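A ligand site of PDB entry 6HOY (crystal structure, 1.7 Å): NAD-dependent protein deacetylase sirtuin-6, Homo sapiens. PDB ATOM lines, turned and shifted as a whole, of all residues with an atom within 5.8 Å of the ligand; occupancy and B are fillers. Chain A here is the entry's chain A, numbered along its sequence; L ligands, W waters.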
ATOM      1  N   GLU A  16       2.847  -7.779  -2.955  1.00  0.00           N
ATOM      2  CA  GLU A  16       1.710  -6.845  -3.175  1.00  0.00           C
ATOM      3  C   GLU A  16       1.791  -6.288  -4.598  1.00  0.00           C
ATOM      4  O   GLU A  16       2.940  -6.114  -5.175  1.00  0.00           O
ATOM      5  CB  GLU A  16       1.737  -5.740  -2.141  1.00  0.00           C
ATOM      6  CG  GLU A  16       1.496  -6.301  -0.716  1.00  0.00           C
ATOM      7  CD  GLU A  16       1.452  -5.266   0.344  1.00  0.00           C
ATOM      8  OE1 GLU A  16       2.196  -4.318   0.181  1.00  0.00           O
ATOM      9  OE2 GLU A  16       0.638  -5.433   1.337  1.00  0.00           O
ATOM     10  N   THR A  45     -16.168  -9.453   2.435  1.00  0.00           N
ATOM     11  CA  THR A  45     -15.007  -8.860   3.134  1.00  0.00           C
ATOM     12  C   THR A  45     -14.191  -9.962   3.818  1.00  0.00           C
ATOM     13  O   THR A  45     -14.722 -10.874   4.534  1.00  0.00           O
ATOM     14  CB  THR A  45     -15.439  -7.733   4.079  1.00  0.00           C
ATOM     15  OG1 THR A  45     -16.150  -8.321   5.159  1.00  0.00           O
ATOM     16  CG2 THR A  45     -16.243  -6.646   3.417  1.00  0.00           C
ATOM     17  N   GLY A  46     -12.925  -9.649   3.930  1.00  0.00           N
ATOM     18  CA  GLY A  46     -11.941 -10.336   4.751  1.00  0.00           C
ATOM     19  C   GLY A  46     -10.960  -9.385   5.424  1.00  0.00           C
ATOM     20  O   GLY A  46     -11.303  -8.224   5.599  1.00  0.00           O
ATOM     21  N   ALA A  47      -9.893 -10.009   5.979  1.00  0.00           N
ATOM     22  CA  ALA A  47      -9.054  -9.441   7.057  1.00  0.00           C
ATOM     23  C   ALA A  47      -8.420  -8.155   6.524  1.00  0.00           C
ATOM     24  O   ALA A  47      -8.100  -7.262   7.399  1.00  0.00           O
ATOM     25  CB  ALA A  47      -8.018 -10.474   7.527  1.00  0.00           C
ATOM     26  N   GLY A  48      -8.225  -7.992   5.202  1.00  0.00           N
ATOM     27  CA  GLY A  48      -7.637  -6.778   4.549  1.00  0.00           C
ATOM     28  C   GLY A  48      -8.428  -5.480   4.884  1.00  0.00           C
ATOM     29  O   GLY A  48      -7.854  -4.357   4.813  1.00  0.00           O
ATOM     30  N   ILE A  49      -9.702  -5.574   5.211  1.00  0.00           N
ATOM     31  CA  ILE A  49     -10.497  -4.342   5.515  1.00  0.00           C
ATOM     32  C   ILE A  49     -10.271  -3.848   6.984  1.00  0.00           C
ATOM     33  O   ILE A  49     -10.912  -2.859   7.395  1.00  0.00           O
ATOM     34  CB  ILE A  49     -11.989  -4.508   5.146  1.00  0.00           C
ATOM     35  CG1 ILE A  49     -12.729  -5.325   6.200  1.00  0.00           C
ATOM     36  CG2 ILE A  49     -12.231  -5.045   3.734  1.00  0.00           C
ATOM     37  CD1 ILE A  49     -14.243  -5.006   6.292  1.00  0.00           C
ATOM     38  N   THR A  51      -6.923  -4.130   8.535  1.00  0.00           N
ATOM     39  CA  THR A  51      -5.471  -3.936   8.732  1.00  0.00           C
ATOM     40  C   THR A  51      -5.267  -2.434   8.991  1.00  0.00           C
ATOM     41  O   THR A  51      -4.402  -2.096   9.800  1.00  0.00           O
ATOM     42  CB  THR A  51      -4.631  -4.425   7.543  1.00  0.00           C
ATOM     43  OG1 THR A  51      -5.098  -3.712   6.399  1.00  0.00           O
ATOM     44  CG2 THR A  51      -4.691  -5.923   7.329  1.00  0.00           C
ATOM     45  N   ALA A  52      -6.039  -1.530   8.424  1.00  0.00           N
ATOM     46  CA  ALA A  52      -5.908  -0.042   8.659  1.00  0.00           C
ATOM     47  C   ALA A  52      -6.465   0.372  10.060  1.00  0.00           C
ATOM     48  O   ALA A  52      -6.309   1.585  10.501  1.00  0.00           O
ATOM     49  CB  ALA A  52      -6.601   0.695   7.506  1.00  0.00           C
ATOM     50  N   ASP A  57      -3.815  -9.064   9.114  1.00  0.00           N
ATOM     51  CA  ASP A  57      -4.496 -10.100   8.276  1.00  0.00           C
ATOM     52  C   ASP A  57      -3.740 -11.421   8.477  1.00  0.00           C
ATOM     53  O   ASP A  57      -3.020 -11.557   9.467  1.00  0.00           O
ATOM     54  CB  ASP A  57      -4.555  -9.523   6.848  1.00  0.00           C
ATOM     55  CG  ASP A  57      -3.270  -9.377   6.085  1.00  0.00           C
ATOM     56  OD1 ASP A  57      -2.241 -10.015   6.477  1.00  0.00           O
ATOM     57  OD2 ASP A  57      -3.323  -8.691   5.078  1.00  0.00           O
ATOM     58  N   PHE A  58      -4.081 -12.470   7.703  1.00  0.00           N
ATOM     59  CA  PHE A  58      -3.563 -13.844   7.832  1.00  0.00           C
ATOM     60  C   PHE A  58      -2.400 -14.064   6.862  1.00  0.00           C
ATOM     61  O   PHE A  58      -1.398 -14.884   7.233  1.00  0.00           O
ATOM     62  CB  PHE A  58      -4.755 -14.770   7.648  1.00  0.00           C
ATOM     63  CG  PHE A  58      -5.718 -14.695   8.798  1.00  0.00           C
ATOM     64  CD1 PHE A  58      -5.469 -15.399   9.968  1.00  0.00           C
ATOM     65  CD2 PHE A  58      -6.838 -13.842   8.725  1.00  0.00           C
ATOM     66  CE1 PHE A  58      -6.345 -15.264  11.034  1.00  0.00           C
ATOM     67  CE2 PHE A  58      -7.747 -13.797   9.744  1.00  0.00           C
ATOM     68  CZ  PHE A  58      -7.486 -14.480  10.898  1.00  0.00           C
ATOM     69  N   ARG A  59      -2.549 -13.545   5.654  1.00  0.00           N
ATOM     70  CA  ARG A  59      -1.681 -14.046   4.520  1.00  0.00           C
ATOM     71  C   ARG A  59      -1.012 -12.889   3.797  1.00  0.00           C
ATOM     72  O   ARG A  59      -0.251 -13.090   2.866  1.00  0.00           O
ATOM     73  CB  ARG A  59      -2.452 -14.900   3.525  1.00  0.00           C
ATOM     74  CG  ARG A  59      -3.046 -16.126   4.146  1.00  0.00           C
ATOM     75  CD  ARG A  59      -3.856 -17.015   3.240  1.00  0.00           C
ATOM     76  NE  ARG A  59      -4.451 -18.107   3.943  1.00  0.00           N
ATOM     77  CZ  ARG A  59      -5.550 -18.018   4.694  1.00  0.00           C
ATOM     78  NH1 ARG A  59      -6.245 -16.880   4.732  1.00  0.00           N
ATOM     79  NH2 ARG A  59      -5.989 -19.063   5.348  1.00  0.00           N
ATOM     80  N   GLY A  60      -1.200 -11.672   4.303  1.00  0.00           N
ATOM     81  CA  GLY A  60      -0.430 -10.503   3.895  1.00  0.00           C
ATOM     82  C   GLY A  60       1.056 -10.619   4.214  1.00  0.00           C
ATOM     83  O   GLY A  60       1.498 -11.512   4.923  1.00  0.00           O
ATOM     84  N   PRO A  61       1.890  -9.630   3.805  1.00  0.00           N
ATOM     85  CA  PRO A  61       3.318  -9.696   4.111  1.00  0.00           C
ATOM     86  C   PRO A  61       3.641  -9.897   5.597  1.00  0.00           C
ATOM     87  O   PRO A  61       4.630 -10.659   5.937  1.00  0.00           O
ATOM     88  CB  PRO A  61       3.832  -8.349   3.603  1.00  0.00           C
ATOM     89  CG  PRO A  61       2.889  -7.988   2.490  1.00  0.00           C
ATOM     90  CD  PRO A  61       1.525  -8.472   2.962  1.00  0.00           C
ATOM     91  N   TRP A  65      -0.369 -15.918   9.493  1.00  0.00           N
ATOM     92  CA  TRP A  65       0.190 -17.204   9.022  1.00  0.00           C
ATOM     93  C   TRP A  65       1.539 -16.966   8.357  1.00  0.00           C
ATOM     94  O   TRP A  65       2.417 -17.837   8.478  1.00  0.00           O
ATOM     95  CB  TRP A  65      -0.777 -17.939   8.108  1.00  0.00           C
ATOM     96  CG  TRP A  65      -2.152 -18.218   8.624  1.00  0.00           C
ATOM     97  CD1 TRP A  65      -3.247 -18.231   7.820  1.00  0.00           C
ATOM     98  CD2 TRP A  65      -2.621 -18.533   9.957  1.00  0.00           C
ATOM     99  NE1 TRP A  65      -4.353 -18.593   8.522  1.00  0.00           N
ATOM    100  CE2 TRP A  65      -4.010 -18.750   9.844  1.00  0.00           C
ATOM    101  CE3 TRP A  65      -2.016 -18.717  11.200  1.00  0.00           C
ATOM    102  CZ2 TRP A  65      -4.809 -19.087  10.936  1.00  0.00           C
ATOM    103  CZ3 TRP A  65      -2.801 -19.037  12.283  1.00  0.00           C
ATOM    104  CH2 TRP A  65      -4.199 -19.190  12.154  1.00  0.00           C
ATOM    105  N   GLN A 107     -15.718 -13.033   6.363  1.00  0.00           N
ATOM    106  CA  GLN A 107     -14.890 -14.062   6.985  1.00  0.00           C
ATOM    107  C   GLN A 107     -14.355 -13.568   8.332  1.00  0.00           C
ATOM    108  O   GLN A 107     -13.677 -14.294   8.995  1.00  0.00           O
ATOM    109  CB  GLN A 107     -13.799 -14.452   5.986  1.00  0.00           C
ATOM    110  CG  GLN A 107     -14.382 -15.136   4.745  1.00  0.00           C
ATOM    111  CD  GLN A 107     -13.387 -15.374   3.664  1.00  0.00           C
ATOM    112  OE1 GLN A 107     -12.582 -16.286   3.807  1.00  0.00           O
ATOM    113  NE2 GLN A 107     -13.479 -14.575   2.596  1.00  0.00           N
ATOM    114  N   ASN A 108     -14.459 -12.283   8.601  1.00  0.00           N
ATOM    115  CA  ASN A 108     -13.773 -11.679   9.745  1.00  0.00           C
ATOM    116  C   ASN A 108     -14.420 -12.104  11.041  1.00  0.00           C
ATOM    117  O   ASN A 108     -15.684 -12.100  11.178  1.00  0.00           O
ATOM    118  CB  ASN A 108     -13.725 -10.173   9.557  1.00  0.00           C
ATOM    119  CG  ASN A 108     -13.015  -9.814   8.274  1.00  0.00           C
ATOM    120  OD1 ASN A 108     -12.297 -10.618   7.648  1.00  0.00           O
ATOM    121  ND2 ASN A 108     -13.151  -8.573   7.877  1.00  0.00           N
ATOM    122  N   VAL A 109     -13.590 -12.435  11.995  1.00  0.00           N
ATOM    123  CA  VAL A 109     -14.054 -12.570  13.372  1.00  0.00           C
ATOM    124  C   VAL A 109     -13.925 -11.306  14.250  1.00  0.00           C
ATOM    125  O   VAL A 109     -14.168 -11.432  15.530  1.00  0.00           O
ATOM    126  CB  VAL A 109     -13.296 -13.763  13.982  1.00  0.00           C
ATOM    127  CG1 VAL A 109     -13.592 -15.069  13.296  1.00  0.00           C
ATOM    128  CG2 VAL A 109     -11.816 -13.583  14.153  1.00  0.00           C
ATOM    129  N   HIS A 127     -17.180 -17.173   9.719  1.00  0.00           N
ATOM    130  CA  HIS A 127     -16.154 -17.776  10.632  1.00  0.00           C
ATOM    131  C   HIS A 127     -16.381 -17.451  12.115  1.00  0.00           C
ATOM    132  O   HIS A 127     -15.601 -17.982  12.954  1.00  0.00           O
ATOM    133  CB  HIS A 127     -14.743 -17.420  10.111  1.00  0.00           C
ATOM    134  CG  HIS A 127     -14.507 -17.836   8.692  1.00  0.00           C
ATOM    135  ND1 HIS A 127     -13.430 -17.430   7.915  1.00  0.00           N
ATOM    136  CD2 HIS A 127     -15.204 -18.693   7.908  1.00  0.00           C
ATOM    137  CE1 HIS A 127     -13.547 -17.901   6.698  1.00  0.00           C
ATOM    138  NE2 HIS A 127     -14.563 -18.775   6.711  1.00  0.00           N
ATOM    139  N   TRP A 182     -10.444 -25.244  12.646  1.00  0.00           N
ATOM    140  CA  TRP A 182     -10.154 -25.701  11.263  1.00  0.00           C
ATOM    141  C   TRP A 182     -11.159 -26.775  10.809  1.00  0.00           C
ATOM    142  O   TRP A 182     -11.599 -26.699   9.668  1.00  0.00           O
ATOM    143  CB  TRP A 182      -8.720 -26.222  11.137  1.00  0.00           C
ATOM    144  CG  TRP A 182      -7.715 -25.120  11.091  1.00  0.00           C
ATOM    145  CD1 TRP A 182      -6.941 -24.659  12.127  1.00  0.00           C
ATOM    146  CD2 TRP A 182      -7.400 -24.283   9.955  1.00  0.00           C
ATOM    147  NE1 TRP A 182      -6.135 -23.629  11.695  1.00  0.00           N
ATOM    148  CE2 TRP A 182      -6.407 -23.374  10.379  1.00  0.00           C
ATOM    149  CE3 TRP A 182      -7.829 -24.254   8.629  1.00  0.00           C
ATOM    150  CZ2 TRP A 182      -5.860 -22.419   9.511  1.00  0.00           C
ATOM    151  CZ3 TRP A 182      -7.280 -23.317   7.774  1.00  0.00           C
ATOM    152  CH2 TRP A 182      -6.320 -22.401   8.220  1.00  0.00           C
ATOM    153  N   GLY A 208     -10.325  -7.034   0.388  1.00  0.00           N
ATOM    154  CA  GLY A 208      -9.357  -7.538   1.387  1.00  0.00           C
ATOM    155  C   GLY A 208      -9.589  -8.970   1.778  1.00  0.00           C
ATOM    156  O   GLY A 208      -9.466  -9.205   2.934  1.00  0.00           O
ATOM    157  N   THR A 209      -9.867  -9.869   0.810  1.00  0.00           N
ATOM    158  CA  THR A 209      -9.768 -11.332   0.991  1.00  0.00           C
ATOM    159  C   THR A 209      -9.022 -11.968  -0.199  1.00  0.00           C
ATOM    160  O   THR A 209      -9.211 -11.519  -1.329  1.00  0.00           O
ATOM    161  CB  THR A 209     -11.169 -11.941   1.142  1.00  0.00           C
ATOM    162  OG1 THR A 209     -11.002 -13.349   1.126  1.00  0.00           O
ATOM    163  CG2 THR A 209     -12.102 -11.553   0.042  1.00  0.00           C
ATOM    164  N   SER A 210      -8.133 -12.890   0.107  1.00  0.00           N
ATOM    165  CA  SER A 210      -7.318 -13.664  -0.844  1.00  0.00           C
ATOM    166  C   SER A 210      -8.196 -14.806  -1.453  1.00  0.00           C
ATOM    167  O   SER A 210      -7.737 -15.439  -2.370  1.00  0.00           O
ATOM    168  CB  SER A 210      -6.029 -14.147  -0.160  1.00  0.00           C
ATOM    169  OG  SER A 210      -6.342 -15.122   0.771  1.00  0.00           O
ATOM    170  N   LEU A 211      -9.378 -15.056  -0.885  1.00  0.00           N
ATOM    171  CA  LEU A 211     -10.402 -15.990  -1.456  1.00  0.00           C
ATOM    172  C   LEU A 211      -9.870 -17.451  -1.517  1.00  0.00           C
ATOM    173  O   LEU A 211     -10.440 -18.296  -2.279  1.00  0.00           O
ATOM    174  CB  LEU A 211     -10.755 -15.524  -2.874  1.00  0.00           C
ATOM    175  CG  LEU A 211     -11.475 -14.179  -2.984  1.00  0.00           C
ATOM    176  CD1 LEU A 211     -11.607 -13.750  -4.425  1.00  0.00           C
ATOM    177  CD2 LEU A 211     -12.784 -14.200  -2.227  1.00  0.00           C
ATOM    178  N   GLN A 212      -9.019 -17.860  -0.575  1.00  0.00           N
ATOM    179  CA  GLN A 212      -8.337 -19.165  -0.497  1.00  0.00           C
ATOM    180  C   GLN A 212      -9.162 -20.163   0.328  1.00  0.00           C
ATOM    181  O   GLN A 212      -8.804 -21.329   0.221  1.00  0.00           O
ATOM    182  CB  GLN A 212      -6.941 -19.004   0.105  1.00  0.00           C
ATOM    183  CG  GLN A 212      -6.055 -18.086  -0.702  1.00  0.00           C
ATOM    184  CD  GLN A 212      -4.578 -18.195  -0.332  1.00  0.00           C
ATOM    185  OE1 GLN A 212      -4.034 -19.289  -0.339  1.00  0.00           O
ATOM    186  NE2 GLN A 212      -3.880 -17.048  -0.198  1.00  0.00           N
ATOM    187  N   ILE A 213     -10.144 -19.755   1.149  1.00  0.00           N
ATOM    188  CA  ILE A 213     -10.902 -20.676   2.019  1.00  0.00           C
ATOM    189  C   ILE A 213     -12.152 -21.105   1.270  1.00  0.00           C
ATOM    190  O   ILE A 213     -12.909 -20.233   0.819  1.00  0.00           O
ATOM    191  CB  ILE A 213     -11.235 -20.049   3.384  1.00  0.00           C
ATOM    192  CG1 ILE A 213      -9.985 -19.776   4.224  1.00  0.00           C
ATOM    193  CG2 ILE A 213     -12.237 -20.930   4.105  1.00  0.00           C
ATOM    194  CD1 ILE A 213      -9.102 -20.983   4.451  1.00  0.00           C
ATOM    195  N   VAL A 233     -11.146  -6.353  -5.058  1.00  0.00           N
ATOM    196  CA  VAL A 233     -10.202  -5.293  -4.569  1.00  0.00           C
ATOM    197  C   VAL A 233      -9.295  -5.972  -3.567  1.00  0.00           C
ATOM    198  O   VAL A 233      -9.829  -6.491  -2.572  1.00  0.00           O
ATOM    199  CB  VAL A 233     -10.995  -4.165  -3.912  1.00  0.00           C
ATOM    200  CG1 VAL A 233     -10.104  -2.982  -3.522  1.00  0.00           C
ATOM    201  CG2 VAL A 233     -12.160  -3.718  -4.808  1.00  0.00           C
ATOM    202  N   ASN A 234      -7.963  -5.939  -3.795  1.00  0.00           N
ATOM    203  CA  ASN A 234      -6.968  -6.667  -2.954  1.00  0.00           C
ATOM    204  C   ASN A 234      -5.572  -6.197  -3.334  1.00  0.00           C
ATOM    205  O   ASN A 234      -5.319  -6.037  -4.622  1.00  0.00           O
ATOM    206  CB  ASN A 234      -7.154  -8.195  -3.082  1.00  0.00           C
ATOM    207  CG  ASN A 234      -6.758  -8.910  -1.823  1.00  0.00           C
ATOM    208  OD1 ASN A 234      -7.271  -8.610  -0.740  1.00  0.00           O
ATOM    209  ND2 ASN A 234      -5.733  -9.741  -1.885  1.00  0.00           N
ATOM    210  N   LEU A 235      -4.703  -6.018  -2.347  1.00  0.00           N
ATOM    211  CA  LEU A 235      -3.263  -5.735  -2.602  1.00  0.00           C
ATOM    212  C   LEU A 235      -2.528  -6.957  -3.187  1.00  0.00           C
ATOM    213  O   LEU A 235      -1.778  -6.743  -4.166  1.00  0.00           O
ATOM    214  CB  LEU A 235      -2.605  -5.202  -1.319  1.00  0.00           C
ATOM    215  CG  LEU A 235      -3.010  -3.790  -0.895  1.00  0.00           C
ATOM    216  CD1 LEU A 235      -2.350  -3.481   0.441  1.00  0.00           C
ATOM    217  CD2 LEU A 235      -2.628  -2.746  -1.933  1.00  0.00           C
ATOM    218  N   GLN A 236      -2.815  -8.169  -2.731  1.00  0.00           N
ATOM    219  CA  GLN A 236      -2.145  -9.415  -3.231  1.00  0.00           C
ATOM    220  C   GLN A 236      -2.996 -10.045  -4.334  1.00  0.00           C
ATOM    221  O   GLN A 236      -4.150  -9.711  -4.461  1.00  0.00           O
ATOM    222  CB  GLN A 236      -1.968 -10.455  -2.153  1.00  0.00           C
ATOM    223  CG  GLN A 236      -0.842 -10.153  -1.162  1.00  0.00           C
ATOM    224  CD  GLN A 236      -0.807 -11.159  -0.037  1.00  0.00           C
ATOM    225  OE1 GLN A 236      -1.857 -11.642   0.431  1.00  0.00           O
ATOM    226  NE2 GLN A 236       0.368 -11.416   0.534  1.00  0.00           N
ATOM    227  N   PRO A 237      -2.434 -10.911  -5.176  1.00  0.00           N
ATOM    228  CA  PRO A 237      -3.237 -11.822  -5.981  1.00  0.00           C
ATOM    229  C   PRO A 237      -4.219 -12.551  -5.070  1.00  0.00           C
ATOM    230  O   PRO A 237      -3.915 -12.757  -3.923  1.00  0.00           O
ATOM    231  CB  PRO A 237      -2.188 -12.839  -6.548  1.00  0.00           C
ATOM    232  CG  PRO A 237      -0.904 -12.007  -6.559  1.00  0.00           C
ATOM    233  CD  PRO A 237      -0.992 -11.189  -5.308  1.00  0.00           C
ATOM    234  N   THR A 238      -5.302 -13.055  -5.654  1.00  0.00           N
ATOM    235  CA  THR A 238      -6.336 -13.882  -4.985  1.00  0.00           C
ATOM    236  C   THR A 238      -6.557 -15.128  -5.815  1.00  0.00           C
ATOM    237  O   THR A 238      -6.204 -15.005  -7.115  1.00  0.00           O
ATOM    238  CB  THR A 238      -7.669 -13.137  -4.781  1.00  0.00           C
ATOM    239  OG1 THR A 238      -8.354 -13.175  -6.032  1.00  0.00           O
ATOM    240  CG2 THR A 238      -7.439 -11.673  -4.375  1.00  0.00           C
ATOM    241  N   GLY A 250      -5.130  -1.873  -4.674  1.00  0.00           N
ATOM    242  CA  GLY A 250      -4.834  -0.636  -3.931  1.00  0.00           C
ATOM    243  C   GLY A 250      -5.382  -0.772  -2.550  1.00  0.00           C
ATOM    244  O   GLY A 250      -6.028  -1.820  -2.268  1.00  0.00           O
ATOM    245  N   TYR A 251      -5.200   0.238  -1.706  1.00  0.00           N
ATOM    246  CA  TYR A 251      -5.733   0.155  -0.323  1.00  0.00           C
ATOM    247  C   TYR A 251      -7.250   0.247  -0.295  1.00  0.00           C
ATOM    248  O   TYR A 251      -7.772   1.095  -1.034  1.00  0.00           O
ATOM    249  CB  TYR A 251      -5.079   1.247   0.530  1.00  0.00           C
ATOM    250  CG  TYR A 251      -3.623   0.960   0.757  1.00  0.00           C
ATOM    251  CD1 TYR A 251      -3.166   0.107   1.780  1.00  0.00           C
ATOM    252  CD2 TYR A 251      -2.659   1.534  -0.067  1.00  0.00           C
ATOM    253  CE1 TYR A 251      -1.827  -0.101   2.006  1.00  0.00           C
ATOM    254  CE2 TYR A 251      -1.314   1.283   0.112  1.00  0.00           C
ATOM    255  CZ  TYR A 251      -0.889   0.497   1.172  1.00  0.00           C
ATOM    256  OH  TYR A 251       0.422   0.177   1.320  1.00  0.00           O
ATOM    257  N   VAL A 252      -7.916  -0.634   0.461  1.00  0.00           N
ATOM    258  CA  VAL A 252      -9.399  -0.698   0.347  1.00  0.00           C
ATOM    259  C   VAL A 252     -10.019   0.625   0.809  1.00  0.00           C
ATOM    260  O   VAL A 252     -10.942   1.059   0.109  1.00  0.00           O
ATOM    261  CB  VAL A 252     -10.102  -1.897   0.992  1.00  0.00           C
ATOM    262  CG1 VAL A 252      -9.781  -3.157   0.226  1.00  0.00           C
ATOM    263  CG2 VAL A 252      -9.816  -2.024   2.458  1.00  0.00           C
ATOM    264  N   ASP A 253      -9.414   1.349   1.760  1.00  0.00           N
ATOM    265  CA  ASP A 253      -9.934   2.702   2.204  1.00  0.00           C
ATOM    266  C   ASP A 253      -9.815   3.712   1.054  1.00  0.00           C
ATOM    267  O   ASP A 253     -10.790   4.503   0.889  1.00  0.00           O
ATOM    268  CB  ASP A 253      -9.220   3.211   3.466  1.00  0.00           C
ATOM    269  CG  ASP A 253      -9.598   2.545   4.769  1.00  0.00           C
ATOM    270  OD1 ASP A 253     -10.687   1.864   4.811  1.00  0.00           O
ATOM    271  OD2 ASP A 253      -8.790   2.658   5.742  1.00  0.00           O
HETATM  272  N1  LIG L   1      -6.196  -2.817   1.370  1.00  0.00           N
HETATM  273  C1  LIG L   1      -6.331  -3.803   0.452  1.00  0.00           C
HETATM  274  N2  LIG L   1      -5.985  -5.104   0.523  1.00  0.00           N
HETATM  275  C2  LIG L   1      -5.535  -5.376   1.774  1.00  0.00           C
HETATM  276  C3  LIG L   1      -5.314  -4.472   2.789  1.00  0.00           C
HETATM  277  C4  LIG L   1      -5.722  -3.141   2.598  1.00  0.00           C
HETATM  278  N3  LIG L   1      -5.630  -2.223   3.558  1.00  0.00           N
HETATM  279  N4  LIG L   1      -4.808  -5.141   3.902  1.00  0.00           N
HETATM  280  C5  LIG L   1      -4.584  -6.366   3.505  1.00  0.00           C
HETATM  281  N5  LIG L   1      -5.053  -6.576   2.258  1.00  0.00           N
HETATM  282  P1  LIG L   1      -6.147 -13.103   4.054  1.00  0.00           P
HETATM  283  P2  LIG L   1      -9.001 -13.756   4.528  1.00  0.00           P
HETATM  284  C6  LIG L   1      -5.171  -7.890   1.566  1.00  0.00           C
HETATM  285  O1  LIG L   1      -5.893 -14.403   3.429  1.00  0.00           O
HETATM  286  O2  LIG L   1     -10.045 -13.041   5.358  1.00  0.00           O
HETATM  287  C7  LIG L   1      -7.965 -17.524   7.773  1.00  0.00           C
HETATM  288  O3  LIG L   1      -7.404 -18.738   8.273  1.00  0.00           O
HETATM  289  C8  LIG L   1      -3.962  -8.796   1.673  1.00  0.00           C
HETATM  290  O4  LIG L   1      -3.102  -8.692   0.545  1.00  0.00           O
HETATM  291  O5  LIG L   1      -5.060 -12.577   4.918  1.00  0.00           O
HETATM  292  O6  LIG L   1      -9.074 -13.803   3.080  1.00  0.00           O
HETATM  293  C9  LIG L   1      -9.136 -17.086   8.689  1.00  0.00           C
HETATM  294  O7  LIG L   1     -10.079 -18.087   9.080  1.00  0.00           O
HETATM  295  C10 LIG L   1      -4.641 -10.180   1.668  1.00  0.00           C
HETATM  296  O8  LIG L   1      -4.408 -10.683   0.377  1.00  0.00           O
HETATM  297  O9  LIG L   1      -7.564 -13.095   4.916  1.00  0.00           O
HETATM  298  C11 LIG L   1      -9.878 -16.130   7.770  1.00  0.00           C
HETATM  299  O10 LIG L   1     -11.218 -15.821   8.189  1.00  0.00           O
HETATM  300  C12 LIG L   1      -6.134  -9.941   1.893  1.00  0.00           C
HETATM  301  O11 LIG L   1      -6.263  -8.533   2.209  1.00  0.00           O
HETATM  302  C13 LIG L   1      -9.765 -16.882   6.445  1.00  0.00           C
HETATM  303  O12 LIG L   1      -8.515 -17.628   6.471  1.00  0.00           O
HETATM  304  C14 LIG L   1      -6.569 -10.749   3.073  1.00  0.00           C
HETATM  305  O13 LIG L   1      -6.327 -12.134   2.820  1.00  0.00           O
HETATM  306  C15 LIG L   1      -9.805 -16.057   5.195  1.00  0.00           C
HETATM  307  O14 LIG L   1      -8.718 -15.076   5.247  1.00  0.00           O
HETATM  308  O   HOH W   1      -8.861 -21.083   8.160  1.00  0.00           O
HETATM  309  O   HOH W   2      -1.348  -7.105   4.366  1.00  0.00           O
HETATM  310  O   HOH W   3     -11.182 -13.910  10.974  1.00  0.00           O
HETATM  311  O   HOH W   4     -10.909 -13.013   7.849  1.00  0.00           O
HETATM  312  O   HOH W   5      -7.436   0.347   3.754  1.00  0.00           O
HETATM  313  O   HOH W   6      -1.233  -7.180   1.506  1.00  0.00           O
HETATM  314  O   HOH W   7     -10.881 -17.591  11.589  1.00  0.00           O
HETATM  315  O   HOH W   8      -8.402 -16.299   2.016  1.00  0.00           O
HETATM  316  O   HOH W   9      -7.621  -1.832   6.061  1.00  0.00           O
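ND2 of Asn 108 is in hydrogen-bond range of O of Gly 46. The backbone carbonyl oxygen (O) of Thr 45 sits at hydrogen-bond distance from the backbone NH (N) of Gln 107, 3.0 Å away. The backbone NH (N) of Leu 211 is in hydrogen-bond range of the side-chain hydroxyl (OG1) of Thr 209 (3.1 Å). OD1 of Asp 57 lies within hydrogen-bond range of N of Gly 60, 2.9 Å away. O of Gly 208 is in hydrogen-bond range of N of Gly 48. OG1 of Thr 51 is in hydrogen-bond range of O of Gly 48, 3.2 Å away. NE2 of Gln 212 sits at hydrogen-bond distance from OG of Ser 210, at 3.3 Å. The backbone NH (N) of Trp 65 is in hydrogen-bond range of the backbone carbonyl oxygen (O) of Phe 58, at 2.7 Å.
An oxygen (O11) of the ligand sits close to the backbone carbonyl oxygen (O) of Gly 208 (3.4 Å). Merely in contact with the ligand: Asp 57 (3.1 Å), Gly 46 (3.4 Å), Gly 250 (3.4 Å), Ile 213 (3.4 Å), Tyr 251 (3.5 Å) and Trp 182 (3.8 Å). 21 residues have an atom within 4 Å of the ligand: Gly 46, Ala 47, Gly 48, Thr 51, Asp 57, Phe 58, Arg 59, Trp 65, Gln 107, His 127, Trp 182, Gly 208, Thr 209, Ser 210, Ile 213, Asn 234, Leu 235, Gln 236, Gly 250, Tyr 251 and Val 252.
O5 of the ligand is in hydrogen-bond range of N of Phe 58, 3.0 Å away. The backbone NH of Arg 59 sits at hydrogen-bond distance from an oxygen (O5) of the ligand (2.8 Å). OE1 of Gln 236 lies within hydrogen-bond range of O8 of the ligand (2.7 Å). NE1 of Trp 65 sits at hydrogen-bond distance from O3 of the ligand, at 3.1 Å. The guanidinium group (NH1) of Arg 59 lies within salt-bridge range of an oxygen (O1) of the ligand (2.8 Å). N of Val 252 is in hydrogen-bond range of N1 of the ligand. An oxygen (O10) of the ligand sits at hydrogen-bond distance from a ring nitrogen (ND1) of His 127, 2.7 Å away. The backbone NH (N) of Gln 236 lies close to an oxygen (O4) of the ligand (3.3 Å). An oxygen (O6) of the ligand sits at hydrogen-bond distance from the side-chain hydroxyl of Thr 209 (2.8 Å). An oxygen (O10) of the ligand sits at hydrogen-bond distance from the backbone carbonyl oxygen of Gln 107 (3.0 Å). The backbone NH of Leu 235 sits at hydrogen-bond distance from a nitrogen (N2) of the ligand (3.3 Å). OG1 of Thr 51 lies within hydrogen-bond range of N4 of the ligand. The backbone NH (N) of Ser 210 lies within hydrogen-bond range of an oxygen (O6) of the ligand, 3.2 Å away. N of Ala 47 is in hydrogen-bond range of O2 of the ligand (3.1 Å). O8 of the ligand sits at hydrogen-bond distance from ND2 of Asn 234, 2.8 Å away. An oxygen (O1) of the ligand is in hydrogen-bond range of the side-chain hydroxyl of Ser 210, 2.8 Å away. The backbone carbonyl oxygen of Gly 48 lies close to a nitrogen (N3) of the ligand (3.3 Å).
Water W6 lies within hydrogen-bond range of the side-chain carboxylate (OE2) of Glu 16 and an oxygen (O4) of the ligand. Water W4 lies within hydrogen-bond range of an oxygen (O2) of the ligand, the side-chain amide oxygen of Asn 108 and the backbone carbonyl oxygen of Gln 107. Water W8 lies within hydrogen-bond range of the side-chain hydroxyl (OG) of Ser 210 (2.7 Å), an oxygen (O6) of the ligand (2.8 Å), the backbone NH (N) of Gln 212 (3.1 Å) and the backbone NH (N) of Leu 211 (3.3 Å). Water W9 lies within hydrogen-bond range of O of Gly 48 (2.8 Å), N of Ala 52 (2.9 Å), OG1 of Thr 51 (3.2 Å) and N3 of the ligand (3.2 Å). Water W3 lies within hydrogen-bond range of the backbone NH of Val 109 (3.0 Å), the backbone carbonyl oxygen of Gln 107 (3.2 Å) and an oxygen (O10) of the ligand (3.4 Å).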
